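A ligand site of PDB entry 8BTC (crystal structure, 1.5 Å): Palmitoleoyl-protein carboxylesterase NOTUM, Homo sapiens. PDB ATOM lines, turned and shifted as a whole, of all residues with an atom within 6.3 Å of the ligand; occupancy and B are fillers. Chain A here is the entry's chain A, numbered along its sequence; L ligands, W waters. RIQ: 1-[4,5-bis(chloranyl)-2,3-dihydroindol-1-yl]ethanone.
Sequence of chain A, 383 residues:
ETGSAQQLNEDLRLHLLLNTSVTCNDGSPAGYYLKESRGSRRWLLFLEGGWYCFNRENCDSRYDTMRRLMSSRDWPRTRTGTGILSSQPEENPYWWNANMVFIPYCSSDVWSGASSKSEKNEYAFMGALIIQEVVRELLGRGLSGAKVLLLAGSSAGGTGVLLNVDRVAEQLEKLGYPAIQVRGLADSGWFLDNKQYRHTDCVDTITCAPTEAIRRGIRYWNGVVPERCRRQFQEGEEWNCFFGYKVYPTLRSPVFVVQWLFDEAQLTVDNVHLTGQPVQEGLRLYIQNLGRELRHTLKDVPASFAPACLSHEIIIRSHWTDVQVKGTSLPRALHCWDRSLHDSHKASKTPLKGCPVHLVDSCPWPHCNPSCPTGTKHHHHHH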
ATOM      1  N   GLY A  49      23.203 -14.806  26.671  1.00  0.00           N
ATOM      2  CA  GLY A  49      22.785 -16.180  26.464  1.00  0.00           C
ATOM      3  C   GLY A  49      21.612 -16.580  27.343  1.00  0.00           C
ATOM      4  O   GLY A  49      20.959 -15.749  27.973  1.00  0.00           O
ATOM      5  N   GLY A  50      21.354 -17.886  27.369  1.00  0.00           N
ATOM      6  CA  GLY A  50      20.253 -18.435  28.138  1.00  0.00           C
ATOM      7  C   GLY A  50      19.489 -19.552  27.467  1.00  0.00           C
ATOM      8  O   GLY A  50      18.258 -19.520  27.412  1.00  0.00           O
ATOM      9  N   TRP A  51      20.206 -20.579  26.980  1.00  0.00           N
ATOM     10  CA  TRP A  51      19.618 -21.763  26.350  1.00  0.00           C
ATOM     11  C   TRP A  51      18.731 -21.309  25.182  1.00  0.00           C
ATOM     12  O   TRP A  51      19.175 -20.465  24.381  1.00  0.00           O
ATOM     13  CB  TRP A  51      18.933 -22.612  27.408  1.00  0.00           C
ATOM     14  CG  TRP A  51      19.893 -23.283  28.331  1.00  0.00           C
ATOM     15  CD1 TRP A  51      20.321 -22.823  29.543  1.00  0.00           C
ATOM     16  CD2 TRP A  51      20.546 -24.556  28.136  1.00  0.00           C
ATOM     17  NE1 TRP A  51      21.206 -23.718  30.105  1.00  0.00           N
ATOM     18  CE2 TRP A  51      21.362 -24.784  29.271  1.00  0.00           C
ATOM     19  CE3 TRP A  51      20.525 -25.507  27.117  1.00  0.00           C
ATOM     20  CZ2 TRP A  51      22.141 -25.929  29.410  1.00  0.00           C
ATOM     21  CZ3 TRP A  51      21.305 -26.649  27.266  1.00  0.00           C
ATOM     22  CH2 TRP A  51      22.101 -26.854  28.395  1.00  0.00           C
ATOM     23  N   TYR A  52      17.519 -21.856  25.040  1.00  0.00           N
ATOM     24  CA  TYR A  52      16.687 -21.778  23.841  1.00  0.00           C
ATOM     25  C   TYR A  52      15.449 -22.616  24.131  1.00  0.00           C
ATOM     26  O   TYR A  52      15.388 -23.341  25.126  1.00  0.00           O
ATOM     27  CB  TYR A  52      17.405 -22.300  22.578  1.00  0.00           C
ATOM     28  CG  TYR A  52      18.187 -23.580  22.826  1.00  0.00           C
ATOM     29  CD1 TYR A  52      17.540 -24.810  22.964  1.00  0.00           C
ATOM     30  CD2 TYR A  52      19.570 -23.566  22.919  1.00  0.00           C
ATOM     31  CE1 TYR A  52      18.263 -25.980  23.214  1.00  0.00           C
ATOM     32  CE2 TYR A  52      20.295 -24.719  23.175  1.00  0.00           C
ATOM     33  CZ  TYR A  52      19.645 -25.925  23.316  1.00  0.00           C
ATOM     34  OH  TYR A  52      20.408 -27.049  23.556  1.00  0.00           O
ATOM     35  N   VAL A 110      18.954 -18.933  19.816  1.00  0.00           N
ATOM     36  CA  VAL A 110      20.398 -18.843  19.643  1.00  0.00           C
ATOM     37  C   VAL A 110      20.730 -17.704  18.674  1.00  0.00           C
ATOM     38  O   VAL A 110      21.707 -17.768  17.924  1.00  0.00           O
ATOM     39  CB  VAL A 110      21.016 -20.171  19.152  1.00  0.00           C
ATOM     40  CG1 VAL A 110      22.538 -20.193  19.388  1.00  0.00           C
ATOM     41  CG2 VAL A 110      20.354 -21.379  19.827  1.00  0.00           C
ATOM     42  N   SER A 155      27.676 -18.006  25.931  1.00  0.00           N
ATOM     43  CA  SER A 155      26.827 -19.201  25.861  1.00  0.00           C
ATOM     44  C   SER A 155      26.014 -19.138  24.579  1.00  0.00           C
ATOM     45  O   SER A 155      26.629 -19.079  23.498  1.00  0.00           O
ATOM     46  CB  SER A 155      26.017 -19.343  27.157  1.00  0.00           C
ATOM     47  OG  SER A 155      25.506 -20.665  27.254  1.00  0.00           O
ATOM     48  N   ALA A 156      24.677 -19.165  24.611  1.00  0.00           N
ATOM     49  CA  ALA A 156      23.954 -19.085  23.354  1.00  0.00           C
ATOM     50  C   ALA A 156      24.259 -17.769  22.628  1.00  0.00           C
ATOM     51  O   ALA A 156      24.207 -17.718  21.395  1.00  0.00           O
ATOM     52  CB  ALA A 156      22.448 -19.259  23.575  1.00  0.00           C
ATOM     53  N   GLY A 157      24.624 -16.712  23.383  1.00  0.00           N
ATOM     54  CA  GLY A 157      25.107 -15.487  22.759  1.00  0.00           C
ATOM     55  C   GLY A 157      26.443 -15.657  22.070  1.00  0.00           C
ATOM     56  O   GLY A 157      26.725 -14.987  21.053  1.00  0.00           O
ATOM     57  N   THR A 159      27.424 -18.512  20.627  1.00  0.00           N
ATOM     58  CA  THR A 159      27.073 -19.121  19.347  1.00  0.00           C
ATOM     59  C   THR A 159      26.397 -18.093  18.436  1.00  0.00           C
ATOM     60  O   THR A 159      26.652 -18.066  17.223  1.00  0.00           O
ATOM     61  CB  THR A 159      26.159 -20.334  19.580  1.00  0.00           C
ATOM     62  OG1 THR A 159      26.726 -21.150  20.605  1.00  0.00           O
ATOM     63  CG2 THR A 159      26.007 -21.154  18.323  1.00  0.00           C
ATOM     64  N   SER A 188      32.093 -19.265  25.389  1.00  0.00           N
ATOM     65  CA  SER A 188      31.276 -20.397  25.858  1.00  0.00           C
ATOM     66  C   SER A 188      30.196 -20.798  24.863  1.00  0.00           C
ATOM     67  O   SER A 188      29.150 -21.344  25.241  1.00  0.00           O
ATOM     68  CB  SER A 188      30.648 -20.100  27.205  1.00  0.00           C
ATOM     69  OG  SER A 188      31.666 -19.906  28.171  1.00  0.00           O
ATOM     70  N   GLY A 189      30.459 -20.568  23.570  1.00  0.00           N
ATOM     71  CA  GLY A 189      29.499 -20.885  22.542  1.00  0.00           C
ATOM     72  C   GLY A 189      30.055 -21.847  21.512  1.00  0.00           C
ATOM     73  O   GLY A 189      29.539 -21.959  20.397  1.00  0.00           O
ATOM     74  N   PHE A 191      30.580 -25.508  20.847  1.00  0.00           N
ATOM     75  CA  PHE A 191      30.059 -26.790  21.294  1.00  0.00           C
ATOM     76  C   PHE A 191      30.476 -27.918  20.360  1.00  0.00           C
ATOM     77  O   PHE A 191      30.747 -27.722  19.183  1.00  0.00           O
ATOM     78  CB  PHE A 191      28.524 -26.742  21.412  1.00  0.00           C
ATOM     79  CG  PHE A 191      28.063 -25.798  22.478  1.00  0.00           C
ATOM     80  CD1 PHE A 191      28.222 -26.124  23.809  1.00  0.00           C
ATOM     81  CD2 PHE A 191      27.547 -24.560  22.145  1.00  0.00           C
ATOM     82  CE1 PHE A 191      27.835 -25.225  24.805  1.00  0.00           C
ATOM     83  CE2 PHE A 191      27.152 -23.667  23.144  1.00  0.00           C
ATOM     84  CZ  PHE A 191      27.301 -24.005  24.459  1.00  0.00           C
ATOM     85  N   LEU A 192      30.504 -29.116  20.916  1.00  0.00           N
ATOM     86  CA  LEU A 192      30.727 -30.326  20.132  1.00  0.00           C
ATOM     87  C   LEU A 192      29.422 -31.117  19.979  1.00  0.00           C
ATOM     88  O   LEU A 192      28.682 -31.309  20.952  1.00  0.00           O
ATOM     89  CB  LEU A 192      31.809 -31.204  20.788  1.00  0.00           C
ATOM     90  CG  LEU A 192      33.142 -30.524  21.060  1.00  0.00           C
ATOM     91  CD1 LEU A 192      34.075 -31.493  21.767  1.00  0.00           C
ATOM     92  CD2 LEU A 192      33.815 -29.971  19.794  1.00  0.00           C
ATOM     93  N   CYS A 208      17.841 -33.258  24.590  1.00  0.00           N
ATOM     94  CA  CYS A 208      18.967 -32.560  25.213  1.00  0.00           C
ATOM     95  C   CYS A 208      20.252 -32.683  24.388  1.00  0.00           C
ATOM     96  O   CYS A 208      21.084 -31.770  24.395  1.00  0.00           O
ATOM     97  CB  CYS A 208      19.197 -33.089  26.624  1.00  0.00           C
ATOM     98  SG  CYS A 208      19.110 -31.834  27.938  1.00  0.00           S
ATOM     99  N   PRO A 210      23.013 -32.296  21.788  1.00  0.00           N
ATOM    100  CA  PRO A 210      23.175 -31.061  21.013  1.00  0.00           C
ATOM    101  C   PRO A 210      22.674 -31.146  19.589  1.00  0.00           C
ATOM    102  O   PRO A 210      22.010 -30.215  19.113  1.00  0.00           O
ATOM    103  CB  PRO A 210      24.701 -30.791  21.097  1.00  0.00           C
ATOM    104  CG  PRO A 210      25.321 -32.065  21.588  1.00  0.00           C
ATOM    105  CD  PRO A 210      24.276 -32.741  22.414  1.00  0.00           C
ATOM    106  N   THR A 211      22.918 -32.262  18.908  1.00  0.00           N
ATOM    107  CA  THR A 211      22.582 -32.352  17.485  1.00  0.00           C
ATOM    108  C   THR A 211      21.082 -32.202  17.256  1.00  0.00           C
ATOM    109  O   THR A 211      20.638 -31.411  16.425  1.00  0.00           O
ATOM    110  CB  THR A 211      23.077 -33.682  16.916  1.00  0.00           C
ATOM    111  OG1 THR A 211      24.470 -33.808  17.194  1.00  0.00           O
ATOM    112  CG2 THR A 211      22.862 -33.722  15.428  1.00  0.00           C
ATOM    113  N   ILE A 214      19.291 -28.596  17.910  1.00  0.00           N
ATOM    114  CA  ILE A 214      19.468 -27.579  16.876  1.00  0.00           C
ATOM    115  C   ILE A 214      18.667 -27.930  15.614  1.00  0.00           C
ATOM    116  O   ILE A 214      18.061 -27.049  14.987  1.00  0.00           O
ATOM    117  CB  ILE A 214      20.972 -27.401  16.558  1.00  0.00           C
ATOM    118  CG1 ILE A 214      21.739 -27.036  17.831  1.00  0.00           C
ATOM    119  CG2 ILE A 214      21.149 -26.350  15.492  1.00  0.00           C
ATOM    120  CD1 ILE A 214      21.134 -25.883  18.580  1.00  0.00           C
ATOM    121  N   TRP A 239      21.841 -27.126  10.489  1.00  0.00           N
ATOM    122  CA  TRP A 239      22.149 -27.277  11.902  1.00  0.00           C
ATOM    123  C   TRP A 239      23.657 -27.375  12.154  1.00  0.00           C
ATOM    124  O   TRP A 239      24.141 -26.994  13.216  1.00  0.00           O
ATOM    125  CB  TRP A 239      21.445 -28.517  12.476  1.00  0.00           C
ATOM    126  CG  TRP A 239      21.951 -29.821  11.918  1.00  0.00           C
ATOM    127  CD1 TRP A 239      21.433 -30.524  10.874  1.00  0.00           C
ATOM    128  CD2 TRP A 239      23.078 -30.579  12.391  1.00  0.00           C
ATOM    129  NE1 TRP A 239      22.170 -31.676  10.659  1.00  0.00           N
ATOM    130  CE2 TRP A 239      23.185 -31.723  11.579  1.00  0.00           C
ATOM    131  CE3 TRP A 239      24.002 -30.398  13.427  1.00  0.00           C
ATOM    132  CZ2 TRP A 239      24.182 -32.692  11.778  1.00  0.00           C
ATOM    133  CZ3 TRP A 239      24.986 -31.342  13.609  1.00  0.00           C
ATOM    134  CH2 TRP A 239      25.072 -32.477  12.797  1.00  0.00           C
ATOM    135  N   PHE A 242      25.640 -24.327  13.501  1.00  0.00           N
ATOM    136  CA  PHE A 242      25.597 -23.902  14.896  1.00  0.00           C
ATOM    137  C   PHE A 242      26.773 -24.440  15.692  1.00  0.00           C
ATOM    138  O   PHE A 242      26.878 -24.117  16.888  1.00  0.00           O
ATOM    139  CB  PHE A 242      24.312 -24.359  15.586  1.00  0.00           C
ATOM    140  CG  PHE A 242      23.090 -23.582  15.215  1.00  0.00           C
ATOM    141  CD1 PHE A 242      22.664 -23.485  13.901  1.00  0.00           C
ATOM    142  CD2 PHE A 242      22.328 -22.969  16.209  1.00  0.00           C
ATOM    143  CE1 PHE A 242      21.509 -22.789  13.571  1.00  0.00           C
ATOM    144  CE2 PHE A 242      21.173 -22.270  15.888  1.00  0.00           C
ATOM    145  CZ  PHE A 242      20.773 -22.182  14.552  1.00  0.00           C
ATOM    146  N   PHE A 243      27.638 -25.254  15.092  1.00  0.00           N
ATOM    147  CA  PHE A 243      28.753 -25.834  15.814  1.00  0.00           C
ATOM    148  C   PHE A 243      30.034 -25.134  15.395  1.00  0.00           C
ATOM    149  O   PHE A 243      30.417 -25.149  14.221  1.00  0.00           O
ATOM    150  CB  PHE A 243      28.782 -27.349  15.584  1.00  0.00           C
ATOM    151  CG  PHE A 243      27.667 -28.020  16.279  1.00  0.00           C
ATOM    152  CD1 PHE A 243      27.797 -28.412  17.605  1.00  0.00           C
ATOM    153  CD2 PHE A 243      26.434 -28.148  15.671  1.00  0.00           C
ATOM    154  CE1 PHE A 243      26.735 -28.975  18.278  1.00  0.00           C
ATOM    155  CE2 PHE A 243      25.372 -28.701  16.330  1.00  0.00           C
ATOM    156  CZ  PHE A 243      25.525 -29.129  17.643  1.00  0.00           C
ATOM    157  N   ASP A 263      33.225 -27.370  29.477  1.00  0.00           N
ATOM    158  CA  ASP A 263      32.125 -26.446  29.669  1.00  0.00           C
ATOM    159  C   ASP A 263      30.930 -27.144  30.310  1.00  0.00           C
ATOM    160  O   ASP A 263      30.502 -28.216  29.866  1.00  0.00           O
ATOM    161  CB  ASP A 263      31.726 -25.832  28.338  1.00  0.00           C
ATOM    162  CG  ASP A 263      30.691 -24.740  28.485  1.00  0.00           C
ATOM    163  OD1 ASP A 263      31.078 -23.577  28.703  1.00  0.00           O
ATOM    164  OD2 ASP A 263      29.487 -25.056  28.383  1.00  0.00           O
ATOM    165  N   ALA A 265      27.759 -26.478  30.306  1.00  0.00           N
ATOM    166  CA  ALA A 265      26.593 -26.683  29.449  1.00  0.00           C
ATOM    167  C   ALA A 265      26.841 -27.798  28.448  1.00  0.00           C
ATOM    168  O   ALA A 265      25.922 -28.571  28.130  1.00  0.00           O
ATOM    169  CB  ALA A 265      26.204 -25.386  28.749  1.00  0.00           C
ATOM    170  N   GLN A 266      28.079 -27.917  27.948  1.00  0.00           N
ATOM    171  CA  GLN A 266      28.477 -29.087  27.147  1.00  0.00           C
ATOM    172  C   GLN A 266      28.245 -30.381  27.931  1.00  0.00           C
ATOM    173  O   GLN A 266      27.659 -31.335  27.426  1.00  0.00           O
ATOM    174  CB  GLN A 266      29.954 -28.952  26.741  1.00  0.00           C
ATOM    175  CG  GLN A 266      30.477 -30.116  25.901  1.00  0.00           C
ATOM    176  CD  GLN A 266      29.939 -30.086  24.475  1.00  0.00           C
ATOM    177  OE1 GLN A 266      30.074 -29.086  23.772  1.00  0.00           O
ATOM    178  NE2 GLN A 266      29.331 -31.188  24.055  1.00  0.00           N
ATOM    179  N   VAL A 269      24.317 -31.178  28.297  1.00  0.00           N
ATOM    180  CA  VAL A 269      23.703 -31.802  27.132  1.00  0.00           C
ATOM    181  C   VAL A 269      24.337 -33.153  26.839  1.00  0.00           C
ATOM    182  O   VAL A 269      23.753 -33.955  26.102  1.00  0.00           O
ATOM    183  CB  VAL A 269      23.768 -30.889  25.882  1.00  0.00           C
ATOM    184  CG1 VAL A 269      22.942 -29.630  26.084  1.00  0.00           C
ATOM    185  CG2 VAL A 269      25.203 -30.558  25.491  1.00  0.00           C
ATOM    186  N   HIS A 312      31.310 -22.223  33.354  1.00  0.00           N
ATOM    187  CA  HIS A 312      30.344 -21.835  32.324  1.00  0.00           C
ATOM    188  C   HIS A 312      30.278 -20.314  32.175  1.00  0.00           C
ATOM    189  O   HIS A 312      29.876 -19.638  33.131  1.00  0.00           O
ATOM    190  CB  HIS A 312      28.971 -22.390  32.665  1.00  0.00           C
ATOM    191  CG  HIS A 312      27.930 -22.051  31.651  1.00  0.00           C
ATOM    192  ND1 HIS A 312      26.744 -21.430  31.967  1.00  0.00           N
ATOM    193  CD2 HIS A 312      27.922 -22.216  30.304  1.00  0.00           C
ATOM    194  CE1 HIS A 312      26.033 -21.252  30.866  1.00  0.00           C
ATOM    195  NE2 HIS A 312      26.731 -21.713  29.841  1.00  0.00           N
HETATM  196  C01 RIQ L   1      23.483 -23.508  27.077  1.00  0.00           C
HETATM  197  C02 RIQ L   1      23.486 -23.250  25.587  1.00  0.00           C
HETATM  198  C05 RIQ L   1      24.204 -25.670  25.172  1.00  0.00           C
HETATM  199  C06 RIQ L   1      24.238 -26.511  23.939  1.00  0.00           C
HETATM  200  C07 RIQ L   1      24.250 -25.481  22.817  1.00  0.00           C
HETATM  201  C08 RIQ L   1      24.514 -25.636  21.472  1.00  0.00           C
HETATM  202  C09 RIQ L   1      24.479 -24.563  20.618  1.00  0.00           C
HETATM  203  C10 RIQ L   1      24.197 -23.263  21.061  1.00  0.00           C
HETATM  204  C11 RIQ L   1      23.935 -23.102  22.425  1.00  0.00           C
HETATM  205  C12 RIQ L   1      23.957 -24.271  23.259  1.00  0.00           C
HETATM  206  N04 RIQ L   1      23.800 -24.347  24.720  1.00  0.00           N
HETATM  207  O03 RIQ L   1      23.207 -22.199  25.114  1.00  0.00           O
HETATM  208 CL13 RIQ L   1      24.848 -24.956  18.934  1.00  0.00          CL
HETATM  209 CL14 RIQ L   1      24.871 -27.249  20.835  1.00  0.00          CL
HETATM  210  O   HOH W   1      23.003 -20.300  26.899  1.00  0.00           O
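The backbone NH (N) of Ala 265 lies within hydrogen-bond range of the side-chain carboxylate (OD2) of Asp 263 (3.0 Å). A ring nitrogen (NE2) of His 312 is in hydrogen-bond range of the side-chain hydroxyl (OG) of Ser 155, at 3.0 Å. The side-chain hydroxyl (OG1) of Thr 159 sits at hydrogen-bond distance from the backbone carbonyl oxygen (O) of Gly 189, at 2.9 Å.
N of Ala 156 lies close to O03 of the ligand, at 3.4 Å. An oxygen (O03) of the ligand sits close to the side-chain hydroxyl (OG) of Ser 155.
CD2 of Trp 51 touches C01 of the ligand, at 3.3 Å. Tyr 52 touches the ligand. Val 110 touches the ligand (CG1 to C10, 3.9 Å). Thr 159 touches the ligand. Phe 191 touches the ligand (CE2 to C12, 3.3 Å). Pro 210 touches the ligand. CD1 of Ile 214 touches CL13 of the ligand (3.8 Å). Phe 242 touches the ligand. Phe 243 touches the ligand. Ala 265 touches the ligand. Hydrophobic or aromatic side chains that line the ligand: Trp 51, Tyr 52, Val 110, Ala 156, Phe 191, Pro 210, Ile 214, Phe 242, Phe 243 and Ala 265. Within 4 Å of the ligand: Trp 51, Tyr 52, Val 110, Ser 155, Ala 156, Thr 159, Phe 191, Pro 210, Ile 214, Phe 242, Phe 243 and Ala 265. The nearest printed residue that does not touch the ligand is Val 269 (4.001 Å).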
